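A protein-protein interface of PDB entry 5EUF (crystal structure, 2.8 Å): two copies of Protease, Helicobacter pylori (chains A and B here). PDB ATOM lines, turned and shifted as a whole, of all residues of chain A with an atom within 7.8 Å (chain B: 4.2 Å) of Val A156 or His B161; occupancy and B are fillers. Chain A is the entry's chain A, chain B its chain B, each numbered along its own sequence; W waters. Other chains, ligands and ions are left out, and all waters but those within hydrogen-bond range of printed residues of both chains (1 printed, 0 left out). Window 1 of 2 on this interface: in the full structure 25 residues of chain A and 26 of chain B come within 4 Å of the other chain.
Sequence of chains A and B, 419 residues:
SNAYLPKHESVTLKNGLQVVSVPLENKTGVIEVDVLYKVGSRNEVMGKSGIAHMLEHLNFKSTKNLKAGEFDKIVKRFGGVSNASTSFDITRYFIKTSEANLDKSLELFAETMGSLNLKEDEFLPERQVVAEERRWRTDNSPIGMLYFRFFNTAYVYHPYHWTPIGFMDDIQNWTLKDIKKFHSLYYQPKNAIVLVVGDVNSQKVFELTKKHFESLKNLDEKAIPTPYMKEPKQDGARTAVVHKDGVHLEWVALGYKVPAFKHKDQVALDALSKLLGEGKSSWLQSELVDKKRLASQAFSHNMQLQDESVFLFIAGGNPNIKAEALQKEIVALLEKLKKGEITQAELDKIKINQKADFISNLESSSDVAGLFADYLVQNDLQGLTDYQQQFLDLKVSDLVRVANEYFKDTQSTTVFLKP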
ATOM      1  N   MET A  46      -0.573 -22.007 -11.568  1.00  0.00           N
ATOM      2  CA  MET A  46       0.459 -21.575 -10.628  1.00  0.00           C
ATOM      3  C   MET A  46       0.557 -20.054 -10.599  1.00  0.00           C
ATOM      4  O   MET A  46       0.717 -19.405 -11.632  1.00  0.00           O
ATOM      5  CB  MET A  46       1.813 -22.195 -10.979  1.00  0.00           C
ATOM      6  CG  MET A  46       2.848 -22.059  -9.870  1.00  0.00           C
ATOM      7  SD  MET A  46       4.414 -23.197 -10.114  1.00  0.00           S
ATOM      8  CE  MET A  46       5.135 -22.368 -11.730  1.00  0.00           C
ATOM      9  N   PHE A 151       4.961 -33.694  -4.598  1.00  0.00           N
ATOM     10  CA  PHE A 151       4.232 -33.345  -5.813  1.00  0.00           C
ATOM     11  C   PHE A 151       4.923 -32.212  -6.568  1.00  0.00           C
ATOM     12  O   PHE A 151       4.761 -32.080  -7.778  1.00  0.00           O
ATOM     13  CB  PHE A 151       2.787 -32.977  -5.480  1.00  0.00           C
ATOM     14  CG  PHE A 151       1.929 -34.163  -5.141  1.00  0.00           C
ATOM     15  CD1 PHE A 151       1.366 -34.935  -6.143  1.00  0.00           C
ATOM     16  CD2 PHE A 151       1.694 -34.512  -3.822  1.00  0.00           C
ATOM     17  CE1 PHE A 151       0.579 -36.032  -5.835  1.00  0.00           C
ATOM     18  CE2 PHE A 151       0.908 -35.609  -3.508  1.00  0.00           C
ATOM     19  CZ  PHE A 151       0.350 -36.370  -4.516  1.00  0.00           C
ATOM     20  N   ASN A 152       5.697 -31.403  -5.851  1.00  0.00           N
ATOM     21  CA  ASN A 152       6.553 -30.409  -6.491  1.00  0.00           C
ATOM     22  C   ASN A 152       7.596 -31.077  -7.378  1.00  0.00           C
ATOM     23  O   ASN A 152       7.995 -30.537  -8.410  1.00  0.00           O
ATOM     24  CB  ASN A 152       7.256 -29.536  -5.448  1.00  0.00           C
ATOM     25  CG  ASN A 152       6.338 -28.508  -4.825  1.00  0.00           C
ATOM     26  OD1 ASN A 152       5.123 -28.551  -5.007  1.00  0.00           O
ATOM     27  ND2 ASN A 152       6.919 -27.575  -4.076  1.00  0.00           N
ATOM     28  N   THR A 153       8.035 -32.260  -6.959  1.00  0.00           N
ATOM     29  CA  THR A 153       9.112 -32.969  -7.635  1.00  0.00           C
ATOM     30  C   THR A 153       8.585 -33.943  -8.686  1.00  0.00           C
ATOM     31  O   THR A 153       9.143 -34.053  -9.778  1.00  0.00           O
ATOM     32  CB  THR A 153       9.980 -33.740  -6.622  1.00  0.00           C
ATOM     33  OG1 THR A 153      10.350 -32.867  -5.548  1.00  0.00           O
ATOM     34  CG2 THR A 153      11.238 -34.284  -7.285  1.00  0.00           C
ATOM     35  N   ALA A 154       7.508 -34.643  -8.347  1.00  0.00           N
ATOM     36  CA  ALA A 154       6.957 -35.675  -9.218  1.00  0.00           C
ATOM     37  C   ALA A 154       6.325 -35.085 -10.472  1.00  0.00           C
ATOM     38  O   ALA A 154       6.350 -35.702 -11.537  1.00  0.00           O
ATOM     39  CB  ALA A 154       5.939 -36.517  -8.459  1.00  0.00           C
ATOM     40  N   TYR A 155       5.753 -33.891 -10.339  1.00  0.00           N
ATOM     41  CA  TYR A 155       5.102 -33.219 -11.460  1.00  0.00           C
ATOM     42  C   TYR A 155       5.773 -31.885 -11.753  1.00  0.00           C
ATOM     43  O   TYR A 155       6.037 -31.098 -10.845  1.00  0.00           O
ATOM     44  CB  TYR A 155       3.614 -32.998 -11.180  1.00  0.00           C
ATOM     45  CG  TYR A 155       2.823 -34.270 -10.983  1.00  0.00           C
ATOM     46  CD1 TYR A 155       2.149 -34.863 -12.045  1.00  0.00           C
ATOM     47  CD2 TYR A 155       2.744 -34.876  -9.736  1.00  0.00           C
ATOM     48  CE1 TYR A 155       1.421 -36.024 -11.871  1.00  0.00           C
ATOM     49  CE2 TYR A 155       2.018 -36.037  -9.551  1.00  0.00           C
ATOM     50  CZ  TYR A 155       1.359 -36.606 -10.621  1.00  0.00           C
ATOM     51  OH  TYR A 155       0.638 -37.762 -10.440  1.00  0.00           O
ATOM     52  N   VAL A 156       6.033 -31.631 -13.027  1.00  0.00           N
ATOM     53  CA  VAL A 156       6.744 -30.428 -13.436  1.00  0.00           C
ATOM     54  C   VAL A 156       5.813 -29.407 -14.086  1.00  0.00           C
ATOM     55  O   VAL A 156       5.969 -28.197 -13.907  1.00  0.00           O
ATOM     56  CB  VAL A 156       7.883 -30.782 -14.409  1.00  0.00           C
ATOM     57  CG1 VAL A 156       8.501 -29.526 -14.999  1.00  0.00           C
ATOM     58  CG2 VAL A 156       8.934 -31.622 -13.698  1.00  0.00           C
ATOM     59  N   TYR A 157       4.823 -29.901 -14.821  1.00  0.00           N
ATOM     60  CA  TYR A 157       4.013 -29.046 -15.671  1.00  0.00           C
ATOM     61  C   TYR A 157       2.526 -29.126 -15.324  1.00  0.00           C
ATOM     62  O   TYR A 157       1.846 -28.101 -15.237  1.00  0.00           O
ATOM     63  CB  TYR A 157       4.259 -29.422 -17.136  1.00  0.00           C
ATOM     64  CG  TYR A 157       3.462 -28.636 -18.143  1.00  0.00           C
ATOM     65  CD1 TYR A 157       3.291 -27.265 -18.009  1.00  0.00           C
ATOM     66  CD2 TYR A 157       2.899 -29.265 -19.245  1.00  0.00           C
ATOM     67  CE1 TYR A 157       2.563 -26.546 -18.936  1.00  0.00           C
ATOM     68  CE2 TYR A 157       2.175 -28.554 -20.181  1.00  0.00           C
ATOM     69  CZ  TYR A 157       2.009 -27.197 -20.020  1.00  0.00           C
ATOM     70  OH  TYR A 157       1.287 -26.488 -20.949  1.00  0.00           O
ATOM     71  N   HIS A 158       2.028 -30.341 -15.123  1.00  0.00           N
ATOM     72  CA  HIS A 158       0.625 -30.552 -14.774  1.00  0.00           C
ATOM     73  C   HIS A 158       0.317 -29.957 -13.399  1.00  0.00           C
ATOM     74  O   HIS A 158       1.179 -29.958 -12.518  1.00  0.00           O
ATOM     75  CB  HIS A 158       0.294 -32.046 -14.803  1.00  0.00           C
ATOM     76  CG  HIS A 158      -1.151 -32.356 -14.571  1.00  0.00           C
ATOM     77  ND1 HIS A 158      -1.668 -32.604 -13.317  1.00  0.00           N
ATOM     78  CD2 HIS A 158      -2.191 -32.454 -15.432  1.00  0.00           C
ATOM     79  CE1 HIS A 158      -2.964 -32.841 -13.417  1.00  0.00           C
ATOM     80  NE2 HIS A 158      -3.306 -32.755 -14.689  1.00  0.00           N
ATOM     81  N   PRO A 159      -0.909 -29.435 -13.213  1.00  0.00           N
ATOM     82  CA  PRO A 159      -1.325 -28.824 -11.943  1.00  0.00           C
ATOM     83  C   PRO A 159      -1.147 -29.707 -10.706  1.00  0.00           C
ATOM     84  O   PRO A 159      -1.315 -29.209  -9.592  1.00  0.00           O
ATOM     85  CB  PRO A 159      -2.804 -28.525 -12.180  1.00  0.00           C
ATOM     86  CG  PRO A 159      -2.875 -28.238 -13.631  1.00  0.00           C
ATOM     87  CD  PRO A 159      -1.897 -29.187 -14.278  1.00  0.00           C
ATOM     88  N   TYR A 160      -0.801 -30.980 -10.883  1.00  0.00           N
ATOM     89  CA  TYR A 160      -0.455 -31.829  -9.745  1.00  0.00           C
ATOM     90  C   TYR A 160       0.921 -31.441  -9.210  1.00  0.00           C
ATOM     91  O   TYR A 160       1.452 -32.080  -8.304  1.00  0.00           O
ATOM     92  CB  TYR A 160      -0.478 -33.313 -10.128  1.00  0.00           C
ATOM     93  CG  TYR A 160      -1.858 -33.867 -10.408  1.00  0.00           C
ATOM     94  CD1 TYR A 160      -3.000 -33.169 -10.038  1.00  0.00           C
ATOM     95  CD2 TYR A 160      -2.017 -35.094 -11.040  1.00  0.00           C
ATOM     96  CE1 TYR A 160      -4.264 -33.675 -10.295  1.00  0.00           C
ATOM     97  CE2 TYR A 160      -3.274 -35.607 -11.301  1.00  0.00           C
ATOM     98  CZ  TYR A 160      -4.393 -34.894 -10.925  1.00  0.00           C
ATOM     99  OH  TYR A 160      -5.644 -35.405 -11.182  1.00  0.00           O
ATOM    100  N   HIS A 161       1.488 -30.386  -9.788  1.00  0.00           N
ATOM    101  CA  HIS A 161       2.739 -29.804  -9.323  1.00  0.00           C
ATOM    102  C   HIS A 161       2.585 -29.274  -7.901  1.00  0.00           C
ATOM    103  O   HIS A 161       3.569 -29.115  -7.180  1.00  0.00           O
ATOM    104  CB  HIS A 161       3.183 -28.685 -10.271  1.00  0.00           C
ATOM    105  CG  HIS A 161       4.499 -28.064  -9.913  1.00  0.00           C
ATOM    106  ND1 HIS A 161       5.670 -28.789  -9.838  1.00  0.00           N
ATOM    107  CD2 HIS A 161       4.830 -26.784  -9.623  1.00  0.00           C
ATOM    108  CE1 HIS A 161       6.664 -27.983  -9.511  1.00  0.00           C
ATOM    109  NE2 HIS A 161       6.182 -26.761  -9.374  1.00  0.00           N
ATOM    110  N   TRP A 162       1.346 -29.003  -7.501  1.00  0.00           N
ATOM    111  CA  TRP A 162       1.070 -28.510  -6.156  1.00  0.00           C
ATOM    112  C   TRP A 162      -0.136 -29.189  -5.512  1.00  0.00           C
ATOM    113  O   TRP A 162      -1.010 -29.731  -6.190  1.00  0.00           O
ATOM    114  CB  TRP A 162       0.852 -26.995  -6.176  1.00  0.00           C
ATOM    115  CG  TRP A 162      -0.350 -26.565  -6.966  1.00  0.00           C
ATOM    116  CD1 TRP A 162      -1.628 -26.431  -6.506  1.00  0.00           C
ATOM    117  CD2 TRP A 162      -0.382 -26.209  -8.354  1.00  0.00           C
ATOM    118  NE1 TRP A 162      -2.455 -26.017  -7.522  1.00  0.00           N
ATOM    119  CE2 TRP A 162      -1.715 -25.872  -8.666  1.00  0.00           C
ATOM    120  CE3 TRP A 162       0.585 -26.142  -9.362  1.00  0.00           C
ATOM    121  CZ2 TRP A 162      -2.105 -25.476  -9.944  1.00  0.00           C
ATOM    122  CZ3 TRP A 162       0.197 -25.747 -10.630  1.00  0.00           C
ATOM    123  CH2 TRP A 162      -1.137 -25.419 -10.910  1.00  0.00           C
ATOM    124  N   MET A 229      -2.495 -28.841 -19.687  1.00  0.00           N
ATOM    125  CA  MET A 229      -1.128 -29.107 -19.252  1.00  0.00           C
ATOM    126  C   MET A 229      -0.916 -30.584 -18.938  1.00  0.00           C
ATOM    127  O   MET A 229      -1.045 -31.010 -17.792  1.00  0.00           O
ATOM    128  CB  MET A 229      -0.777 -28.260 -18.027  1.00  0.00           C
ATOM    129  CG  MET A 229      -1.934 -27.443 -17.481  1.00  0.00           C
ATOM    130  SD  MET A 229      -1.726 -25.549 -17.867  1.00  0.00           S
ATOM    131  CE  MET A 229      -3.410 -24.902 -17.128  1.00  0.00           C
ATOM    132  N   LYS A 230      -0.585 -31.360 -19.964  1.00  0.00           N
ATOM    133  CA  LYS A 230      -0.342 -32.789 -19.801  1.00  0.00           C
ATOM    134  C   LYS A 230       1.096 -33.047 -19.360  1.00  0.00           C
ATOM    135  O   LYS A 230       2.037 -32.531 -19.967  1.00  0.00           O
ATOM    136  CB  LYS A 230      -0.644 -33.530 -21.107  1.00  0.00           C
ATOM    137  CG  LYS A 230      -0.456 -35.036 -21.041  1.00  0.00           C
ATOM    138  CD  LYS A 230      -0.674 -35.670 -22.409  1.00  0.00           C
ATOM    139  CE  LYS A 230      -0.552 -37.189 -22.351  1.00  0.00           C
ATOM    140  NZ  LYS A 230      -1.637 -37.808 -21.540  1.00  0.00           N
ATOM    141  N   GLU A 231       1.267 -33.835 -18.302  1.00  0.00           N
ATOM    142  CA  GLU A 231       2.603 -34.188 -17.830  1.00  0.00           C
ATOM    143  C   GLU A 231       3.352 -34.993 -18.875  1.00  0.00           C
ATOM    144  O   GLU A 231       2.873 -36.036 -19.320  1.00  0.00           O
ATOM    145  CB  GLU A 231       2.541 -34.989 -16.531  1.00  0.00           C
ATOM    146  CG  GLU A 231       2.899 -34.202 -15.291  1.00  0.00           C
ATOM    147  CD  GLU A 231       4.271 -33.573 -15.359  1.00  0.00           C
ATOM    148  OE1 GLU A 231       5.245 -34.280 -15.697  1.00  0.00           O
ATOM    149  OE2 GLU A 231       4.374 -32.364 -15.069  1.00  0.00           O
ATOM    150  N   PRO A 232       4.531 -34.507 -19.277  1.00  0.00           N
ATOM    151  CA  PRO A 232       5.376 -35.325 -20.147  1.00  0.00           C
ATOM    152  C   PRO A 232       5.758 -36.611 -19.424  1.00  0.00           C
ATOM    153  O   PRO A 232       5.923 -36.581 -18.204  1.00  0.00           O
ATOM    154  CB  PRO A 232       6.598 -34.433 -20.397  1.00  0.00           C
ATOM    155  CG  PRO A 232       6.122 -33.036 -20.113  1.00  0.00           C
ATOM    156  CD  PRO A 232       5.121 -33.185 -19.006  1.00  0.00           C
ATOM    157  N   ASP A 235      11.099 -39.386 -17.451  1.00  0.00           N
ATOM    158  CA  ASP A 235      12.216 -39.890 -18.237  1.00  0.00           C
ATOM    159  C   ASP A 235      13.407 -40.304 -17.380  1.00  0.00           C
ATOM    160  O   ASP A 235      14.534 -40.369 -17.868  1.00  0.00           O
ATOM    161  CB  ASP A 235      12.648 -38.820 -19.241  1.00  0.00           C
ATOM    162  CG  ASP A 235      12.474 -37.406 -18.697  1.00  0.00           C
ATOM    163  OD1 ASP A 235      12.349 -37.249 -17.463  1.00  0.00           O
ATOM    164  OD2 ASP A 235      12.463 -36.452 -19.501  1.00  0.00           O
ATOM    165  N   ARG A 238      13.652 -38.735 -10.254  1.00  0.00           N
ATOM    166  CA  ARG A 238      13.737 -37.384  -9.712  1.00  0.00           C
ATOM    167  C   ARG A 238      13.834 -37.459  -8.195  1.00  0.00           C
ATOM    168  O   ARG A 238      13.104 -38.223  -7.564  1.00  0.00           O
ATOM    169  CB  ARG A 238      12.522 -36.551 -10.131  1.00  0.00           C
ATOM    170  CG  ARG A 238      12.314 -36.485 -11.634  1.00  0.00           C
ATOM    171  CD  ARG A 238      10.970 -35.879 -12.001  1.00  0.00           C
ATOM    172  NE  ARG A 238      10.728 -35.978 -13.440  1.00  0.00           N
ATOM    173  CZ  ARG A 238       9.591 -35.635 -14.038  1.00  0.00           C
ATOM    174  NH1 ARG A 238       8.576 -35.168 -13.327  1.00  0.00           N
ATOM    175  NH2 ARG A 238       9.468 -35.764 -15.352  1.00  0.00           N
ATOM    176  N   LYS A 257       5.111 -43.144 -10.892  1.00  0.00           N
ATOM    177  CA  LYS A 257       4.078 -42.672 -11.809  1.00  0.00           C
ATOM    178  C   LYS A 257       3.120 -43.798 -12.172  1.00  0.00           C
ATOM    179  O   LYS A 257       3.537 -44.931 -12.421  1.00  0.00           O
ATOM    180  CB  LYS A 257       4.700 -42.080 -13.074  1.00  0.00           C
ATOM    181  CG  LYS A 257       5.277 -40.686 -12.894  1.00  0.00           C
ATOM    182  CD  LYS A 257       4.187 -39.656 -12.664  1.00  0.00           C
ATOM    183  CE  LYS A 257       4.748 -38.244 -12.733  1.00  0.00           C
ATOM    184  NZ  LYS A 257       5.347 -37.938 -14.065  1.00  0.00           N
ATOM    185  N   MET B  46       2.898 -20.192 -15.873  1.00  0.00           N
ATOM    186  CA  MET B  46       2.818 -21.541 -16.428  1.00  0.00           C
ATOM    187  C   MET B  46       1.408 -21.849 -16.924  1.00  0.00           C
ATOM    188  O   MET B  46       0.428 -21.692 -16.198  1.00  0.00           O
ATOM    189  CB  MET B  46       3.259 -22.581 -15.401  1.00  0.00           C
ATOM    190  CG  MET B  46       3.557 -23.940 -16.016  1.00  0.00           C
ATOM    191  SD  MET B  46       4.502 -25.151 -14.812  1.00  0.00           S
ATOM    192  CE  MET B  46       3.160 -25.280 -13.407  1.00  0.00           C
ATOM    193  N   PHE B 151      16.198 -26.095 -15.246  1.00  0.00           N
ATOM    194  CA  PHE B 151      15.448 -25.025 -14.605  1.00  0.00           C
ATOM    195  C   PHE B 151      14.120 -25.528 -14.043  1.00  0.00           C
ATOM    196  O   PHE B 151      13.604 -24.975 -13.073  1.00  0.00           O
ATOM    197  CB  PHE B 151      15.225 -23.869 -15.581  1.00  0.00           C
ATOM    198  CG  PHE B 151      16.429 -22.985 -15.750  1.00  0.00           C
ATOM    199  CD1 PHE B 151      16.700 -21.981 -14.836  1.00  0.00           C
ATOM    200  CD2 PHE B 151      17.297 -23.164 -16.816  1.00  0.00           C
ATOM    201  CE1 PHE B 151      17.812 -21.166 -14.984  1.00  0.00           C
ATOM    202  CE2 PHE B 151      18.412 -22.352 -16.970  1.00  0.00           C
ATOM    203  CZ  PHE B 151      18.669 -21.353 -16.053  1.00  0.00           C
ATOM    204  N   ASN B 152      13.577 -26.582 -14.645  1.00  0.00           N
ATOM    205  CA  ASN B 152      12.405 -27.252 -14.087  1.00  0.00           C
ATOM    206  C   ASN B 152      12.699 -27.809 -12.698  1.00  0.00           C
ATOM    207  O   ASN B 152      11.831 -27.825 -11.824  1.00  0.00           O
ATOM    208  CB  ASN B 152      11.933 -28.390 -14.997  1.00  0.00           C
ATOM    209  CG  ASN B 152      11.401 -27.898 -16.325  1.00  0.00           C
ATOM    210  OD1 ASN B 152      11.375 -28.642 -17.307  1.00  0.00           O
ATOM    211  ND2 ASN B 152      10.972 -26.641 -16.364  1.00  0.00           N
ATOM    212  N   TYR B 155      14.271 -24.637  -9.984  1.00  0.00           N
ATOM    213  CA  TYR B 155      13.204 -23.745  -9.541  1.00  0.00           C
ATOM    214  C   TYR B 155      11.863 -24.470  -9.557  1.00  0.00           C
ATOM    215  O   TYR B 155      11.580 -25.257 -10.461  1.00  0.00           O
ATOM    216  CB  TYR B 155      13.129 -22.498 -10.422  1.00  0.00           C
ATOM    217  CG  TYR B 155      14.350 -21.604 -10.373  1.00  0.00           C
ATOM    218  CD1 TYR B 155      14.470 -20.607  -9.410  1.00  0.00           C
ATOM    219  CD2 TYR B 155      15.372 -21.738 -11.305  1.00  0.00           C
ATOM    220  CE1 TYR B 155      15.573 -19.777  -9.367  1.00  0.00           C
ATOM    221  CE2 TYR B 155      16.483 -20.911 -11.271  1.00  0.00           C
ATOM    222  CZ  TYR B 155      16.576 -19.933 -10.301  1.00  0.00           C
ATOM    223  OH  TYR B 155      17.680 -19.110 -10.265  1.00  0.00           O
ATOM    224  N   VAL B 156      11.036 -24.193  -8.559  1.00  0.00           N
ATOM    225  CA  VAL B 156       9.768 -24.894  -8.401  1.00  0.00           C
ATOM    226  C   VAL B 156       8.588 -23.939  -8.545  1.00  0.00           C
ATOM    227  O   VAL B 156       7.537 -24.299  -9.075  1.00  0.00           O
ATOM    228  CB  VAL B 156       9.700 -25.596  -7.029  1.00  0.00           C
ATOM    229  CG1 VAL B 156       8.362 -26.285  -6.838  1.00  0.00           C
ATOM    230  CG2 VAL B 156      10.840 -26.592  -6.892  1.00  0.00           C
ATOM    231  N   HIS B 158       9.087 -19.941  -8.740  1.00  0.00           N
ATOM    232  CA  HIS B 158       9.437 -18.755  -9.516  1.00  0.00           C
ATOM    233  C   HIS B 158       9.400 -19.064 -11.014  1.00  0.00           C
ATOM    234  O   HIS B 158       9.693 -20.187 -11.421  1.00  0.00           O
ATOM    235  CB  HIS B 158      10.819 -18.250  -9.096  1.00  0.00           C
ATOM    236  CG  HIS B 158      11.192 -16.929  -9.686  1.00  0.00           C
ATOM    237  ND1 HIS B 158      11.961 -16.813 -10.824  1.00  0.00           N
ATOM    238  CD2 HIS B 158      10.908 -15.665  -9.293  1.00  0.00           C
ATOM    239  CE1 HIS B 158      12.132 -15.534 -11.107  1.00  0.00           C
ATOM    240  NE2 HIS B 158      11.503 -14.817 -10.193  1.00  0.00           N
ATOM    241  N   PRO B 159       9.020 -18.073 -11.840  1.00  0.00           N
ATOM    242  CA  PRO B 159       8.961 -18.236 -13.299  1.00  0.00           C
ATOM    243  C   PRO B 159      10.254 -18.739 -13.954  1.00  0.00           C
ATOM    244  O   PRO B 159      10.221 -19.126 -15.121  1.00  0.00           O
ATOM    245  CB  PRO B 159       8.635 -16.825 -13.784  1.00  0.00           C
ATOM    246  CG  PRO B 159       7.818 -16.258 -12.694  1.00  0.00           C
ATOM    247  CD  PRO B 159       8.402 -16.804 -11.416  1.00  0.00           C
ATOM    248  N   TYR B 160      11.364 -18.753 -13.221  1.00  0.00           N
ATOM    249  CA  TYR B 160      12.598 -19.343 -13.735  1.00  0.00           C
ATOM    250  C   TYR B 160      12.481 -20.865 -13.777  1.00  0.00           C
ATOM    251  O   TYR B 160      13.432 -21.562 -14.131  1.00  0.00           O
ATOM    252  CB  TYR B 160      13.804 -18.930 -12.887  1.00  0.00           C
ATOM    253  CG  TYR B 160      14.187 -17.472 -13.012  1.00  0.00           C
ATOM    254  CD1 TYR B 160      13.664 -16.677 -14.024  1.00  0.00           C
ATOM    255  CD2 TYR B 160      15.080 -16.892 -12.119  1.00  0.00           C
ATOM    256  CE1 TYR B 160      14.015 -15.342 -14.138  1.00  0.00           C
ATOM    257  CE2 TYR B 160      15.438 -15.561 -12.226  1.00  0.00           C
ATOM    258  CZ  TYR B 160      14.903 -14.792 -13.236  1.00  0.00           C
ATOM    259  OH  TYR B 160      15.259 -13.468 -13.345  1.00  0.00           O
ATOM    260  N   HIS B 161      11.305 -21.366 -13.408  1.00  0.00           N
ATOM    261  CA  HIS B 161      10.971 -22.782 -13.512  1.00  0.00           C
ATOM    262  C   HIS B 161      11.069 -23.262 -14.958  1.00  0.00           C
ATOM    263  O   HIS B 161      11.278 -24.446 -15.220  1.00  0.00           O
ATOM    264  CB  HIS B 161       9.563 -23.026 -12.964  1.00  0.00           C
ATOM    265  CG  HIS B 161       9.152 -24.465 -12.949  1.00  0.00           C
ATOM    266  ND1 HIS B 161       9.750 -25.403 -12.134  1.00  0.00           N
ATOM    267  CD2 HIS B 161       8.189 -25.124 -13.636  1.00  0.00           C
ATOM    268  CE1 HIS B 161       9.177 -26.578 -12.326  1.00  0.00           C
ATOM    269  NE2 HIS B 161       8.228 -26.437 -13.233  1.00  0.00           N
ATOM    270  N   TRP B 162      10.914 -22.331 -15.893  1.00  0.00           N
ATOM    271  CA  TRP B 162      11.032 -22.638 -17.313  1.00  0.00           C
ATOM    272  C   TRP B 162      11.889 -21.601 -18.040  1.00  0.00           C
ATOM    273  O   TRP B 162      11.951 -20.435 -17.646  1.00  0.00           O
ATOM    274  CB  TRP B 162       9.648 -22.724 -17.961  1.00  0.00           C
ATOM    275  CG  TRP B 162       8.863 -21.441 -17.902  1.00  0.00           C
ATOM    276  CD1 TRP B 162       8.867 -20.436 -18.825  1.00  0.00           C
ATOM    277  CD2 TRP B 162       7.963 -21.029 -16.865  1.00  0.00           C
ATOM    278  NE1 TRP B 162       8.027 -19.425 -18.428  1.00  0.00           N
ATOM    279  CE2 TRP B 162       7.460 -19.763 -17.229  1.00  0.00           C
ATOM    280  CE3 TRP B 162       7.535 -21.606 -15.666  1.00  0.00           C
ATOM    281  CZ2 TRP B 162       6.549 -19.066 -16.437  1.00  0.00           C
ATOM    282  CZ3 TRP B 162       6.631 -20.914 -14.882  1.00  0.00           C
ATOM    283  CH2 TRP B 162       6.148 -19.657 -15.271  1.00  0.00           C
HETATM  284  O   HOH W   1       9.806 -28.965 -10.055  1.00  0.00           O
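Met A46 touches its own counterpart, Met B46.
Met A46 touches Val B156, and with the chains exchanged Val A156 touches Met B46.
Met A46 touches Trp B162, but with the chains exchanged Trp A162 does not touch Met B46 (4.1 Å).
Asn A152 touches Val B156, and with the chains exchanged Val A156 touches Asn B152.
Positions printed for both chains: 46, 151, 152, 155, 156, 158, 159, 160, 161 and 162.
Among the printed residues, pairs that only touch across the chains: Asn A152 with Val B156 (3.4 Å), Val A156 with Asn B152 (3.6 Å), Tyr A157 with Met B46 (3.6 Å), Met A46 with Trp B162 (3.8 Å) and Met A46 with Met B46 (3.9 Å).
OD1 of Asn A152 lies close to O of His A161, at 2.7 Å.
A ring nitrogen (ND1) of His A161 sits at hydrogen-bond distance from the backbone carbonyl oxygen of Tyr A155 (2.5 Å).
The backbone carbonyl oxygen of His B161 is in hydrogen-bond range of the side-chain amide nitrogen of Asn B152, at 2.5 Å.
A ring nitrogen (ND1) of His B161 lies within hydrogen-bond range of the backbone carbonyl oxygen (O) of Tyr B155 (2.5 Å).
N of Val A156 sits at hydrogen-bond distance from OE2 of Glu A231.
The side-chain carboxylate of Glu A231 sits at hydrogen-bond distance from the backbone NH of Tyr A157 (2.5 Å).
Water W1 bridges O of Asn A152 (2.9 Å) and O of Asn B152 (2.9 Å).
A ring nitrogen (NE2) of His A161 is in hydrogen-bond range of the backbone carbonyl oxygen (O) of Val B156 (2.8 Å).
SD of Met A46 lies close to O of Val B156 (3.5 Å).
O of Val A156 lies within hydrogen-bond range of NE2 of His B161 (2.9 Å).
The backbone carbonyl oxygen of Val A156 sits close to the side-chain sulfur of Met B46, at 3.5 Å.
Val A156 touches three residues of chain B.
His B161 touches one residue of chain A.
Of the printed residues of chain B, Tyr A157 touches Met B46.
Of the printed residues of chain A, Trp B162 touches Met A46.
Of the printed residues of chain B, Asn A152 touches Val B156.
The nearest printed residue of chain B that does not touch Val A156 is Val B156 (6.4 Å).
The nearest residue of chain A that does not touch His B161 is His A161 (4.03 Å).
Printed residues of chain A that touch a printed residue of chain B: Met A46, Asn A152, Val A156, Tyr A157 and His A161.
Hydrophobic or aromatic side chains of chain A within 4 Å of the printed part of chain B: Met A46, Val A156, Tyr A157 and His A161.
Among the printed residues, 9 pairs touch across the chains.
Among the printed residues, no Asp or Glu carboxylate lies within 4 Å of a Lys or Arg side-chain nitrogen of the other chain.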
